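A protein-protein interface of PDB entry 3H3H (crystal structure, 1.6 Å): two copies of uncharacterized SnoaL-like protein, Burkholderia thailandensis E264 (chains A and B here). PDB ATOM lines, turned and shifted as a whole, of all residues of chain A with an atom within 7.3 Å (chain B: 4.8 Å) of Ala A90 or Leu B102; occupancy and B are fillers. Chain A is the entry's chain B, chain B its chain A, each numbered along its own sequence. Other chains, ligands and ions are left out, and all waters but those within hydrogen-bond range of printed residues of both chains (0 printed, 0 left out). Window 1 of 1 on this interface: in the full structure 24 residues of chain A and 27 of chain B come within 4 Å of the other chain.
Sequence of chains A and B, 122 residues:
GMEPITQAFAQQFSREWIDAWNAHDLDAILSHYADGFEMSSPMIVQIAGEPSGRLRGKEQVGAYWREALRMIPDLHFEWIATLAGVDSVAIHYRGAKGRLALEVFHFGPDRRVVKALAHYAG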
ATOM      1  N   ALA A  10     -18.558   3.487  17.035  1.00  0.00           N
ATOM      2  CA  ALA A  10     -19.803   3.986  17.597  1.00  0.00           C
ATOM      3  C   ALA A  10     -19.707   5.467  17.989  1.00  0.00           C
ATOM      4  O   ALA A  10     -20.612   6.270  17.787  1.00  0.00           O
ATOM      5  CB  ALA A  10     -20.184   3.114  18.804  1.00  0.00           C
ATOM      6  N   PHE A  13     -19.139   7.712  14.748  1.00  0.00           N
ATOM      7  CA  PHE A  13     -20.420   7.808  14.088  1.00  0.00           C
ATOM      8  C   PHE A  13     -21.300   8.799  14.857  1.00  0.00           C
ATOM      9  O   PHE A  13     -21.985   9.653  14.294  1.00  0.00           O
ATOM     10  CB  PHE A  13     -21.130   6.446  14.004  1.00  0.00           C
ATOM     11  CG  PHE A  13     -22.555   6.545  13.544  1.00  0.00           C
ATOM     12  CD1 PHE A  13     -22.853   6.740  12.221  1.00  0.00           C
ATOM     13  CD2 PHE A  13     -23.588   6.448  14.446  1.00  0.00           C
ATOM     14  CE1 PHE A  13     -24.164   6.907  11.812  1.00  0.00           C
ATOM     15  CE2 PHE A  13     -24.940   6.586  14.016  1.00  0.00           C
ATOM     16  CZ  PHE A  13     -25.202   6.818  12.739  1.00  0.00           C
ATOM     17  N   SER A  14     -21.395   8.622  16.160  1.00  0.00           N
ATOM     18  CA  SER A  14     -22.244   9.493  16.972  1.00  0.00           C
ATOM     19  C   SER A  14     -21.840  10.982  16.851  1.00  0.00           C
ATOM     20  O   SER A  14     -22.672  11.848  16.700  1.00  0.00           O
ATOM     21  CB  SER A  14     -22.197   9.029  18.422  1.00  0.00           C
ATOM     22  OG  SER A  14     -22.666   7.712  18.535  1.00  0.00           O
ATOM     23  N   TRP A  79     -25.813  15.422  22.542  1.00  0.00           N
ATOM     24  CA  TRP A  79     -25.379  14.036  22.707  1.00  0.00           C
ATOM     25  C   TRP A  79     -25.152  13.658  24.152  1.00  0.00           C
ATOM     26  O   TRP A  79     -24.344  14.287  24.835  1.00  0.00           O
ATOM     27  CB  TRP A  79     -24.127  13.826  21.917  1.00  0.00           C
ATOM     28  CG  TRP A  79     -23.562  12.466  21.906  1.00  0.00           C
ATOM     29  CD1 TRP A  79     -24.207  11.299  22.087  1.00  0.00           C
ATOM     30  CD2 TRP A  79     -22.189  12.128  21.632  1.00  0.00           C
ATOM     31  NE1 TRP A  79     -23.348  10.255  21.991  1.00  0.00           N
ATOM     32  CE2 TRP A  79     -22.091  10.730  21.712  1.00  0.00           C
ATOM     33  CE3 TRP A  79     -21.049  12.870  21.322  1.00  0.00           C
ATOM     34  CZ2 TRP A  79     -20.902  10.047  21.463  1.00  0.00           C
ATOM     35  CZ3 TRP A  79     -19.828  12.188  21.111  1.00  0.00           C
ATOM     36  CH2 TRP A  79     -19.765  10.799  21.203  1.00  0.00           C
ATOM     37  N   ALA A  81     -25.241   9.875  25.337  1.00  0.00           N
ATOM     38  CA  ALA A  81     -24.422   8.675  25.413  1.00  0.00           C
ATOM     39  C   ALA A  81     -24.562   7.863  24.153  1.00  0.00           C
ATOM     40  O   ALA A  81     -25.559   7.961  23.456  1.00  0.00           O
ATOM     41  CB  ALA A  81     -24.907   7.813  26.608  1.00  0.00           C
ATOM     42  N   THR A  82     -23.589   7.001  23.890  1.00  0.00           N
ATOM     43  CA  THR A  82     -23.708   6.072  22.795  1.00  0.00           C
ATOM     44  C   THR A  82     -23.428   4.676  23.323  1.00  0.00           C
ATOM     45  O   THR A  82     -22.468   4.484  24.094  1.00  0.00           O
ATOM     46  CB  THR A  82     -22.713   6.375  21.688  1.00  0.00           C
ATOM     47  OG1 THR A  82     -23.180   7.502  20.958  1.00  0.00           O
ATOM     48  CG2 THR A  82     -22.677   5.234  20.712  1.00  0.00           C
ATOM     49  N   LEU A  83     -24.228   3.723  22.890  1.00  0.00           N
ATOM     50  CA  LEU A  83     -24.067   2.342  23.359  1.00  0.00           C
ATOM     51  C   LEU A  83     -24.012   1.457  22.134  1.00  0.00           C
ATOM     52  O   LEU A  83     -24.684   1.719  21.147  1.00  0.00           O
ATOM     53  CB  LEU A  83     -25.210   1.953  24.239  1.00  0.00           C
ATOM     54  CG  LEU A  83     -25.365   2.920  25.424  1.00  0.00           C
ATOM     55  CD1 LEU A  83     -26.431   3.998  25.097  1.00  0.00           C
ATOM     56  CD2 LEU A  83     -25.748   2.128  26.663  1.00  0.00           C
ATOM     57  N   ALA A  84     -23.152   0.466  22.178  1.00  0.00           N
ATOM     58  CA  ALA A  84     -22.926  -0.397  21.007  1.00  0.00           C
ATOM     59  C   ALA A  84     -23.547  -1.759  21.204  1.00  0.00           C
ATOM     60  O   ALA A  84     -23.406  -2.372  22.241  1.00  0.00           O
ATOM     61  CB  ALA A  84     -21.400  -0.542  20.760  1.00  0.00           C
ATOM     62  N   GLY A  85     -24.174  -2.255  20.135  1.00  0.00           N
ATOM     63  CA  GLY A  85     -24.707  -3.601  20.110  1.00  0.00           C
ATOM     64  C   GLY A  85     -23.983  -4.490  19.119  1.00  0.00           C
ATOM     65  O   GLY A  85     -22.778  -4.413  18.958  1.00  0.00           O
ATOM     66  N   SER A  88     -25.522  -2.692  15.684  1.00  0.00           N
ATOM     67  CA  SER A  88     -26.213  -1.431  15.896  1.00  0.00           C
ATOM     68  C   SER A  88     -25.501  -0.541  16.915  1.00  0.00           C
ATOM     69  O   SER A  88     -24.675  -1.032  17.745  1.00  0.00           O
ATOM     70  CB  SER A  88     -27.641  -1.670  16.320  1.00  0.00           C
ATOM     71  OG  SER A  88     -27.762  -2.491  17.470  1.00  0.00           O
ATOM     72  N   VAL A  89     -25.794   0.747  16.791  1.00  0.00           N
ATOM     73  CA  VAL A  89     -25.348   1.776  17.719  1.00  0.00           C
ATOM     74  C   VAL A  89     -26.610   2.451  18.204  1.00  0.00           C
ATOM     75  O   VAL A  89     -27.532   2.687  17.430  1.00  0.00           O
ATOM     76  CB  VAL A  89     -24.419   2.775  17.021  1.00  0.00           C
ATOM     77  CG1 VAL A  89     -24.116   3.978  17.865  1.00  0.00           C
ATOM     78  CG2 VAL A  89     -23.082   2.062  16.668  1.00  0.00           C
ATOM     79  N   ALA A  90     -26.654   2.787  19.475  1.00  0.00           N
ATOM     80  CA  ALA A  90     -27.784   3.533  20.033  1.00  0.00           C
ATOM     81  C   ALA A  90     -27.266   4.853  20.482  1.00  0.00           C
ATOM     82  O   ALA A  90     -26.306   4.900  21.264  1.00  0.00           O
ATOM     83  CB  ALA A  90     -28.380   2.805  21.256  1.00  0.00           C
ATOM     84  N   ILE A  91     -27.834   5.924  19.948  1.00  0.00           N
ATOM     85  CA  ILE A  91     -27.459   7.264  20.345  1.00  0.00           C
ATOM     86  C   ILE A  91     -28.561   7.813  21.221  1.00  0.00           C
ATOM     87  O   ILE A  91     -29.686   7.933  20.787  1.00  0.00           O
ATOM     88  CB  ILE A  91     -27.232   8.205  19.151  1.00  0.00           C
ATOM     89  CG1 ILE A  91     -26.141   7.631  18.204  1.00  0.00           C
ATOM     90  CG2 ILE A  91     -26.809   9.649  19.647  1.00  0.00           C
ATOM     91  CD1 ILE A  91     -25.823   8.587  16.989  1.00  0.00           C
ATOM     92  N   HIS A  92     -28.190   8.221  22.434  1.00  0.00           N
ATOM     93  CA  HIS A  92     -29.117   8.797  23.394  1.00  0.00           C
ATOM     94  C   HIS A  92     -28.790  10.271  23.362  1.00  0.00           C
ATOM     95  O   HIS A  92     -27.638  10.679  23.528  1.00  0.00           O
ATOM     96  CB  HIS A  92     -28.881   8.125  24.746  1.00  0.00           C
ATOM     97  CG  HIS A  92     -29.726   8.640  25.854  1.00  0.00           C
ATOM     98  ND1 HIS A  92     -31.075   8.886  25.714  1.00  0.00           N
ATOM     99  CD2 HIS A  92     -29.407   8.935  27.135  1.00  0.00           C
ATOM    100  CE1 HIS A  92     -31.551   9.325  26.870  1.00  0.00           C
ATOM    101  NE2 HIS A  92     -30.571   9.331  27.758  1.00  0.00           N
ATOM    102  N   TYR A  93     -29.816  11.074  23.146  1.00  0.00           N
ATOM    103  CA  TYR A  93     -29.601  12.498  23.007  1.00  0.00           C
ATOM    104  C   TYR A  93     -30.839  13.253  23.377  1.00  0.00           C
ATOM    105  O   TYR A  93     -31.901  12.665  23.609  1.00  0.00           O
ATOM    106  CB  TYR A  93     -29.199  12.814  21.565  1.00  0.00           C
ATOM    107  CG  TYR A  93     -30.247  12.564  20.505  1.00  0.00           C
ATOM    108  CD1 TYR A  93     -30.397  11.333  19.915  1.00  0.00           C
ATOM    109  CD2 TYR A  93     -31.040  13.608  19.999  1.00  0.00           C
ATOM    110  CE1 TYR A  93     -31.304  11.152  18.914  1.00  0.00           C
ATOM    111  CE2 TYR A  93     -31.937  13.413  19.005  1.00  0.00           C
ATOM    112  CZ  TYR A  93     -32.063  12.194  18.436  1.00  0.00           C
ATOM    113  OH  TYR A  93     -32.984  12.010  17.410  1.00  0.00           O
ATOM    114  N   LEU A 102     -33.690   8.410  21.906  1.00  0.00           N
ATOM    115  CA  LEU A 102     -32.838   7.237  21.832  1.00  0.00           C
ATOM    116  C   LEU A 102     -33.090   6.605  20.465  1.00  0.00           C
ATOM    117  O   LEU A 102     -34.148   6.050  20.155  1.00  0.00           O
ATOM    118  CB  LEU A 102     -33.138   6.247  22.936  1.00  0.00           C
ATOM    119  CG  LEU A 102     -32.273   5.004  23.044  1.00  0.00           C
ATOM    120  CD1 LEU A 102     -32.224   4.062  21.835  1.00  0.00           C
ATOM    121  CD2 LEU A 102     -30.802   5.431  23.365  1.00  0.00           C
ATOM    122  N   GLU A 103     -32.082   6.745  19.588  1.00  0.00           N
ATOM    123  CA  GLU A 103     -32.174   6.321  18.226  1.00  0.00           C
ATOM    124  C   GLU A 103     -31.233   5.167  18.020  1.00  0.00           C
ATOM    125  O   GLU A 103     -30.056   5.256  18.323  1.00  0.00           O
ATOM    126  CB  GLU A 103     -31.868   7.522  17.291  1.00  0.00           C
ATOM    127  CG  GLU A 103     -32.471   7.453  15.940  1.00  0.00           C
ATOM    128  CD  GLU A 103     -32.935   8.815  15.452  1.00  0.00           C
ATOM    129  OE1 GLU A 103     -32.791   9.091  14.252  1.00  0.00           O
ATOM    130  OE2 GLU A 103     -33.342   9.676  16.261  1.00  0.00           O
ATOM    131  N   VAL A 104     -31.757   4.085  17.454  1.00  0.00           N
ATOM    132  CA  VAL A 104     -30.990   2.891  17.221  1.00  0.00           C
ATOM    133  C   VAL A 104     -30.702   2.820  15.724  1.00  0.00           C
ATOM    134  O   VAL A 104     -31.639   2.935  14.884  1.00  0.00           O
ATOM    135  CB  VAL A 104     -31.765   1.665  17.631  1.00  0.00           C
ATOM    136  CG1 VAL A 104     -30.935   0.435  17.337  1.00  0.00           C
ATOM    137  CG2 VAL A 104     -32.096   1.720  19.176  1.00  0.00           C
ATOM    138  N   PHE A 105     -29.419   2.585  15.404  1.00  0.00           N
ATOM    139  CA  PHE A 105     -28.981   2.529  14.034  1.00  0.00           C
ATOM    140  C   PHE A 105     -28.357   1.203  13.743  1.00  0.00           C
ATOM    141  O   PHE A 105     -27.368   0.799  14.383  1.00  0.00           O
ATOM    142  CB  PHE A 105     -27.926   3.589  13.787  1.00  0.00           C
ATOM    143  CG  PHE A 105     -28.347   4.989  14.160  1.00  0.00           C
ATOM    144  CD1 PHE A 105     -28.189   5.487  15.456  1.00  0.00           C
ATOM    145  CD2 PHE A 105     -28.860   5.852  13.205  1.00  0.00           C
ATOM    146  CE1 PHE A 105     -28.577   6.755  15.768  1.00  0.00           C
ATOM    147  CE2 PHE A 105     -29.246   7.156  13.528  1.00  0.00           C
ATOM    148  CZ  PHE A 105     -29.109   7.613  14.799  1.00  0.00           C
ATOM    149  N   PHE A 107     -26.404  -1.170  11.048  1.00  0.00           N
ATOM    150  CA  PHE A 107     -25.466  -0.928   9.943  1.00  0.00           C
ATOM    151  C   PHE A 107     -25.378  -2.100   9.000  1.00  0.00           C
ATOM    152  O   PHE A 107     -25.523  -3.240   9.427  1.00  0.00           O
ATOM    153  CB  PHE A 107     -24.071  -0.630  10.454  1.00  0.00           C
ATOM    154  CG  PHE A 107     -23.999   0.668  11.155  1.00  0.00           C
ATOM    155  CD1 PHE A 107     -24.429   0.775  12.495  1.00  0.00           C
ATOM    156  CD2 PHE A 107     -23.659   1.804  10.455  1.00  0.00           C
ATOM    157  CE1 PHE A 107     -24.427   2.024  13.109  1.00  0.00           C
ATOM    158  CE2 PHE A 107     -23.670   3.040  11.077  1.00  0.00           C
ATOM    159  CZ  PHE A 107     -24.060   3.129  12.372  1.00  0.00           C
ATOM    160  N   HIS A 119     -36.915   6.659  19.337  1.00  0.00           N
ATOM    161  CA  HIS A 119     -37.655   6.468  20.558  1.00  0.00           C
ATOM    162  C   HIS A 119     -37.576   7.761  21.308  1.00  0.00           C
ATOM    163  O   HIS A 119     -36.531   8.428  21.299  1.00  0.00           O
ATOM    164  CB  HIS A 119     -37.027   5.412  21.458  1.00  0.00           C
ATOM    165  CG  HIS A 119     -36.834   4.078  20.820  1.00  0.00           C
ATOM    166  ND1 HIS A 119     -35.825   3.828  19.909  1.00  0.00           N
ATOM    167  CD2 HIS A 119     -37.480   2.901  21.020  1.00  0.00           C
ATOM    168  CE1 HIS A 119     -35.953   2.571  19.483  1.00  0.00           C
ATOM    169  NE2 HIS A 119     -36.911   1.974  20.188  1.00  0.00           N
ATOM    170  N   ALA B  90     -37.175   1.399  24.743  1.00  0.00           N
ATOM    171  CA  ALA B  90     -35.761   1.417  25.041  1.00  0.00           C
ATOM    172  C   ALA B  90     -35.592   1.739  26.505  1.00  0.00           C
ATOM    173  O   ALA B  90     -36.094   2.765  26.986  1.00  0.00           O
ATOM    174  CB  ALA B  90     -35.031   2.480  24.164  1.00  0.00           C
ATOM    175  N   ILE B  91     -34.928   0.840  27.217  1.00  0.00           N
ATOM    176  CA  ILE B  91     -34.536   1.051  28.591  1.00  0.00           C
ATOM    177  C   ILE B  91     -33.048   1.256  28.752  1.00  0.00           C
ATOM    178  O   ILE B  91     -32.254   0.374  28.465  1.00  0.00           O
ATOM    179  CB  ILE B  91     -35.000  -0.085  29.511  1.00  0.00           C
ATOM    180  CG1 ILE B  91     -36.478  -0.330  29.341  1.00  0.00           C
ATOM    181  CG2 ILE B  91     -34.620   0.235  31.015  1.00  0.00           C
ATOM    182  CD1 ILE B  91     -36.925  -1.524  30.219  1.00  0.00           C
ATOM    183  N   HIS B  92     -32.705   2.442  29.240  1.00  0.00           N
ATOM    184  CA  HIS B  92     -31.346   2.836  29.518  1.00  0.00           C
ATOM    185  C   HIS B  92     -31.116   2.772  31.028  1.00  0.00           C
ATOM    186  O   HIS B  92     -31.918   3.256  31.819  1.00  0.00           O
ATOM    187  CB  HIS B  92     -31.131   4.254  28.968  1.00  0.00           C
ATOM    188  CG  HIS B  92     -29.752   4.808  29.122  1.00  0.00           C
ATOM    189  ND1 HIS B  92     -28.612   4.072  28.890  1.00  0.00           N
ATOM    190  CD2 HIS B  92     -29.340   6.069  29.408  1.00  0.00           C
ATOM    191  CE1 HIS B  92     -27.559   4.857  29.043  1.00  0.00           C
ATOM    192  NE2 HIS B  92     -27.974   6.074  29.352  1.00  0.00           N
ATOM    193  N   TYR B  93     -30.017   2.123  31.396  1.00  0.00           N
ATOM    194  CA  TYR B  93     -29.739   1.816  32.777  1.00  0.00           C
ATOM    195  C   TYR B  93     -28.255   1.573  32.954  1.00  0.00           C
ATOM    196  O   TYR B  93     -27.517   1.388  31.977  1.00  0.00           O
ATOM    197  CB  TYR B  93     -30.569   0.602  33.222  1.00  0.00           C
ATOM    198  CG  TYR B  93     -30.193  -0.661  32.545  1.00  0.00           C
ATOM    199  CD1 TYR B  93     -30.661  -0.966  31.272  1.00  0.00           C
ATOM    200  CD2 TYR B  93     -29.355  -1.595  33.187  1.00  0.00           C
ATOM    201  CE1 TYR B  93     -30.295  -2.160  30.653  1.00  0.00           C
ATOM    202  CE2 TYR B  93     -28.962  -2.758  32.540  1.00  0.00           C
ATOM    203  CZ  TYR B  93     -29.449  -3.051  31.296  1.00  0.00           C
ATOM    204  OH  TYR B  93     -29.054  -4.217  30.651  1.00  0.00           O
ATOM    205  N   LEU B 100     -22.855   1.347  31.592  1.00  0.00           N
ATOM    206  CA  LEU B 100     -24.090   1.847  31.015  1.00  0.00           C
ATOM    207  C   LEU B 100     -24.579   0.872  29.964  1.00  0.00           C
ATOM    208  O   LEU B 100     -23.790   0.320  29.162  1.00  0.00           O
ATOM    209  CB  LEU B 100     -23.972   3.258  30.377  1.00  0.00           C
ATOM    210  CG  LEU B 100     -24.399   4.517  31.173  1.00  0.00           C
ATOM    211  CD1 LEU B 100     -23.954   4.420  32.561  1.00  0.00           C
ATOM    212  CD2 LEU B 100     -23.859   5.785  30.461  1.00  0.00           C
ATOM    213  N   ALA B 101     -25.895   0.775  29.904  1.00  0.00           N
ATOM    214  CA  ALA B 101     -26.519  -0.232  29.095  1.00  0.00           C
ATOM    215  C   ALA B 101     -27.791   0.285  28.504  1.00  0.00           C
ATOM    216  O   ALA B 101     -28.401   1.272  28.988  1.00  0.00           O
ATOM    217  CB  ALA B 101     -26.789  -1.496  29.984  1.00  0.00           C
ATOM    218  N   LEU B 102     -28.223  -0.439  27.490  1.00  0.00           N
ATOM    219  CA  LEU B 102     -29.461  -0.148  26.861  1.00  0.00           C
ATOM    220  C   LEU B 102     -30.018  -1.461  26.377  1.00  0.00           C
ATOM    221  O   LEU B 102     -29.335  -2.371  25.939  1.00  0.00           O
ATOM    222  CB  LEU B 102     -29.277   0.820  25.722  1.00  0.00           C
ATOM    223  CG  LEU B 102     -30.573   1.171  25.002  1.00  0.00           C
ATOM    224  CD1 LEU B 102     -31.117   2.485  25.602  1.00  0.00           C
ATOM    225  CD2 LEU B 102     -30.239   1.231  23.550  1.00  0.00           C
ATOM    226  N   GLU B 103     -31.279  -1.601  26.566  1.00  0.00           N
ATOM    227  CA  GLU B 103     -31.935  -2.762  26.042  1.00  0.00           C
ATOM    228  C   GLU B 103     -33.072  -2.212  25.206  1.00  0.00           C
ATOM    229  O   GLU B 103     -33.808  -1.340  25.686  1.00  0.00           O
ATOM    230  CB  GLU B 103     -32.426  -3.680  27.154  1.00  0.00           C
ATOM    231  CG  GLU B 103     -32.963  -4.955  26.606  1.00  0.00           C
ATOM    232  CD  GLU B 103     -31.887  -6.004  26.392  1.00  0.00           C
ATOM    233  OE1 GLU B 103     -30.827  -5.901  27.015  1.00  0.00           O
ATOM    234  OE2 GLU B 103     -32.135  -6.910  25.595  1.00  0.00           O
ATOM    235  N   VAL B 104     -33.215  -2.695  23.982  1.00  0.00           N
ATOM    236  CA  VAL B 104     -34.315  -2.336  23.120  1.00  0.00           C
ATOM    237  C   VAL B 104     -35.246  -3.533  23.031  1.00  0.00           C
ATOM    238  O   VAL B 104     -34.781  -4.642  22.813  1.00  0.00           O
ATOM    239  CB  VAL B 104     -33.829  -1.951  21.721  1.00  0.00           C
ATOM    240  CG1 VAL B 104     -35.073  -1.621  20.841  1.00  0.00           C
ATOM    241  CG2 VAL B 104     -32.872  -0.776  21.819  1.00  0.00           C
ATOM    242  N   LEU B 117     -32.647  -6.406  22.117  1.00  0.00           N
ATOM    243  CA  LEU B 117     -31.300  -6.168  21.664  1.00  0.00           C
ATOM    244  C   LEU B 117     -30.577  -5.406  22.741  1.00  0.00           C
ATOM    245  O   LEU B 117     -31.023  -4.350  23.160  1.00  0.00           O
ATOM    246  CB  LEU B 117     -31.260  -5.383  20.399  1.00  0.00           C
ATOM    247  CG  LEU B 117     -31.975  -5.980  19.187  1.00  0.00           C
ATOM    248  CD1 LEU B 117     -33.483  -5.603  19.134  1.00  0.00           C
ATOM    249  CD2 LEU B 117     -31.329  -5.552  17.869  1.00  0.00           C
ATOM    250  N   ALA B 118     -29.477  -5.985  23.203  1.00  0.00           N
ATOM    251  CA  ALA B 118     -28.700  -5.332  24.256  1.00  0.00           C
ATOM    252  C   ALA B 118     -27.628  -4.448  23.607  1.00  0.00           C
ATOM    253  O   ALA B 118     -27.048  -4.814  22.591  1.00  0.00           O
ATOM    254  CB  ALA B 118     -28.063  -6.384  25.204  1.00  0.00           C
ATOM    255  N   HIS B 119     -27.320  -3.340  24.268  1.00  0.00           N
ATOM    256  CA  HIS B 119     -26.258  -2.416  23.880  1.00  0.00           C
ATOM    257  C   HIS B 119     -25.561  -1.981  25.144  1.00  0.00           C
ATOM    258  O   HIS B 119     -26.182  -1.872  26.201  1.00  0.00           O
ATOM    259  CB  HIS B 119     -26.757  -1.142  23.138  1.00  0.00           C
ATOM    260  CG  HIS B 119     -27.566  -1.408  21.908  1.00  0.00           C
ATOM    261  ND1 HIS B 119     -28.858  -1.918  21.960  1.00  0.00           N
ATOM    262  CD2 HIS B 119     -27.324  -1.108  20.615  1.00  0.00           C
ATOM    263  CE1 HIS B 119     -29.331  -1.999  20.730  1.00  0.00           C
ATOM    264  NE2 HIS B 119     -28.426  -1.509  19.889  1.00  0.00           N
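O of Leu A102 lies within hydrogen-bond range of ND1 of His A119, at 2.8 Å.
The backbone carbonyl oxygen of Leu B102 sits at hydrogen-bond distance from the backbone NH of His B119, 2.8 Å away.
O of Ala A81 lies within hydrogen-bond range of N of His A92.
The backbone carbonyl oxygen (O) of Val B104 sits at hydrogen-bond distance from the backbone NH (N) of Leu B117 (2.9 Å).
N of Ala B101 lies within hydrogen-bond range of O of Tyr B93 (2.7 Å).
A ring nitrogen (ND1) of His B92 sits at hydrogen-bond distance from the backbone carbonyl oxygen (O) of Ala B101, at 2.8 Å.
Among the printed residues, merely in contact across the chains: Ala A84 with His B119 (3.3 Å), Leu A83 with Ala B101 (3.3 Å), Ala A90 with Leu B102 (3.3 Å), Gly A85 with His B119 (3.4 Å), Gly A85 with Ala B118 (3.6 Å), Leu A83 with His B119 (3.6 Å), Leu A83 with Leu B100 (3.7 Å), His A92 with His B92 (3.7 Å), Leu A83 with Leu B102 (3.7 Å), Leu A102 with Leu B102 (3.7 Å), Val A104 with Val B104 (3.7 Å) and Leu A102 with Ala B90 (3.9 Å).
Ala A90 touches Leu B102, and with the chains exchanged Leu A102 touches Ala B90.
His A92 touches its own counterpart, His B92.
Leu B102 touches its own counterpart, Leu A102.
Val A104 touches its own counterpart, Val B104.
Positions printed for both chains: 90, 91, 92, 93, 102, 103, 104 and 119.
NE2 of His B119 sits at hydrogen-bond distance from OG of Ser A88, at 2.7 Å.
Printed residues of chain B within 4 Å of Ala A84: His B119.
Of the printed residues of chain B, Ala A90 touches Leu B102 (3.3 Å).
Printed residues of chain B within 4 Å of His A92: His B92 (3.7 Å).
Of the printed residues of chain A, Ala B90 touches Leu A102 (3.9 Å).
Of the printed residues of chain A, Leu B100 touches Leu A83.
Of the printed residues of chain A, Ala B101 touches Leu A83.
Printed residues of chain A within 4 Å of Leu B102: Leu A83 (3.7 Å), Ala A90 (3.3 Å) and Leu A102 (3.7 Å).
The nearest printed residue of chain B that does not touch Ala A90 is His B119 (4.1 Å).
The nearest printed residue of chain A that does not touch Leu B102 is Val A104 (4.8 Å).
The nearest printed residue of chain B that does not touch Leu A102 is Val B104 (4.9 Å).
Of the 12 printed residues of chain B, 8 touch a printed residue of chain A.
Printed residues of chain A that touch a printed residue of chain B: Leu A83, Ala A84, Gly A85, Ser A88, Ala A90, His A92, Leu A102 and Val A104.
Hydrophobic or aromatic side chains of chain A within 4 Å of the printed part of chain B: Leu A83, Ala A90, His A92, Leu A102 and Val A104.
Along chain A the printed residues that touch a printed residue of chain B span positions 83 to 104.
Among the printed residues, no Asp or Glu carboxylate lies within 4 Å of a Lys or Arg side-chain nitrogen of the other chain.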
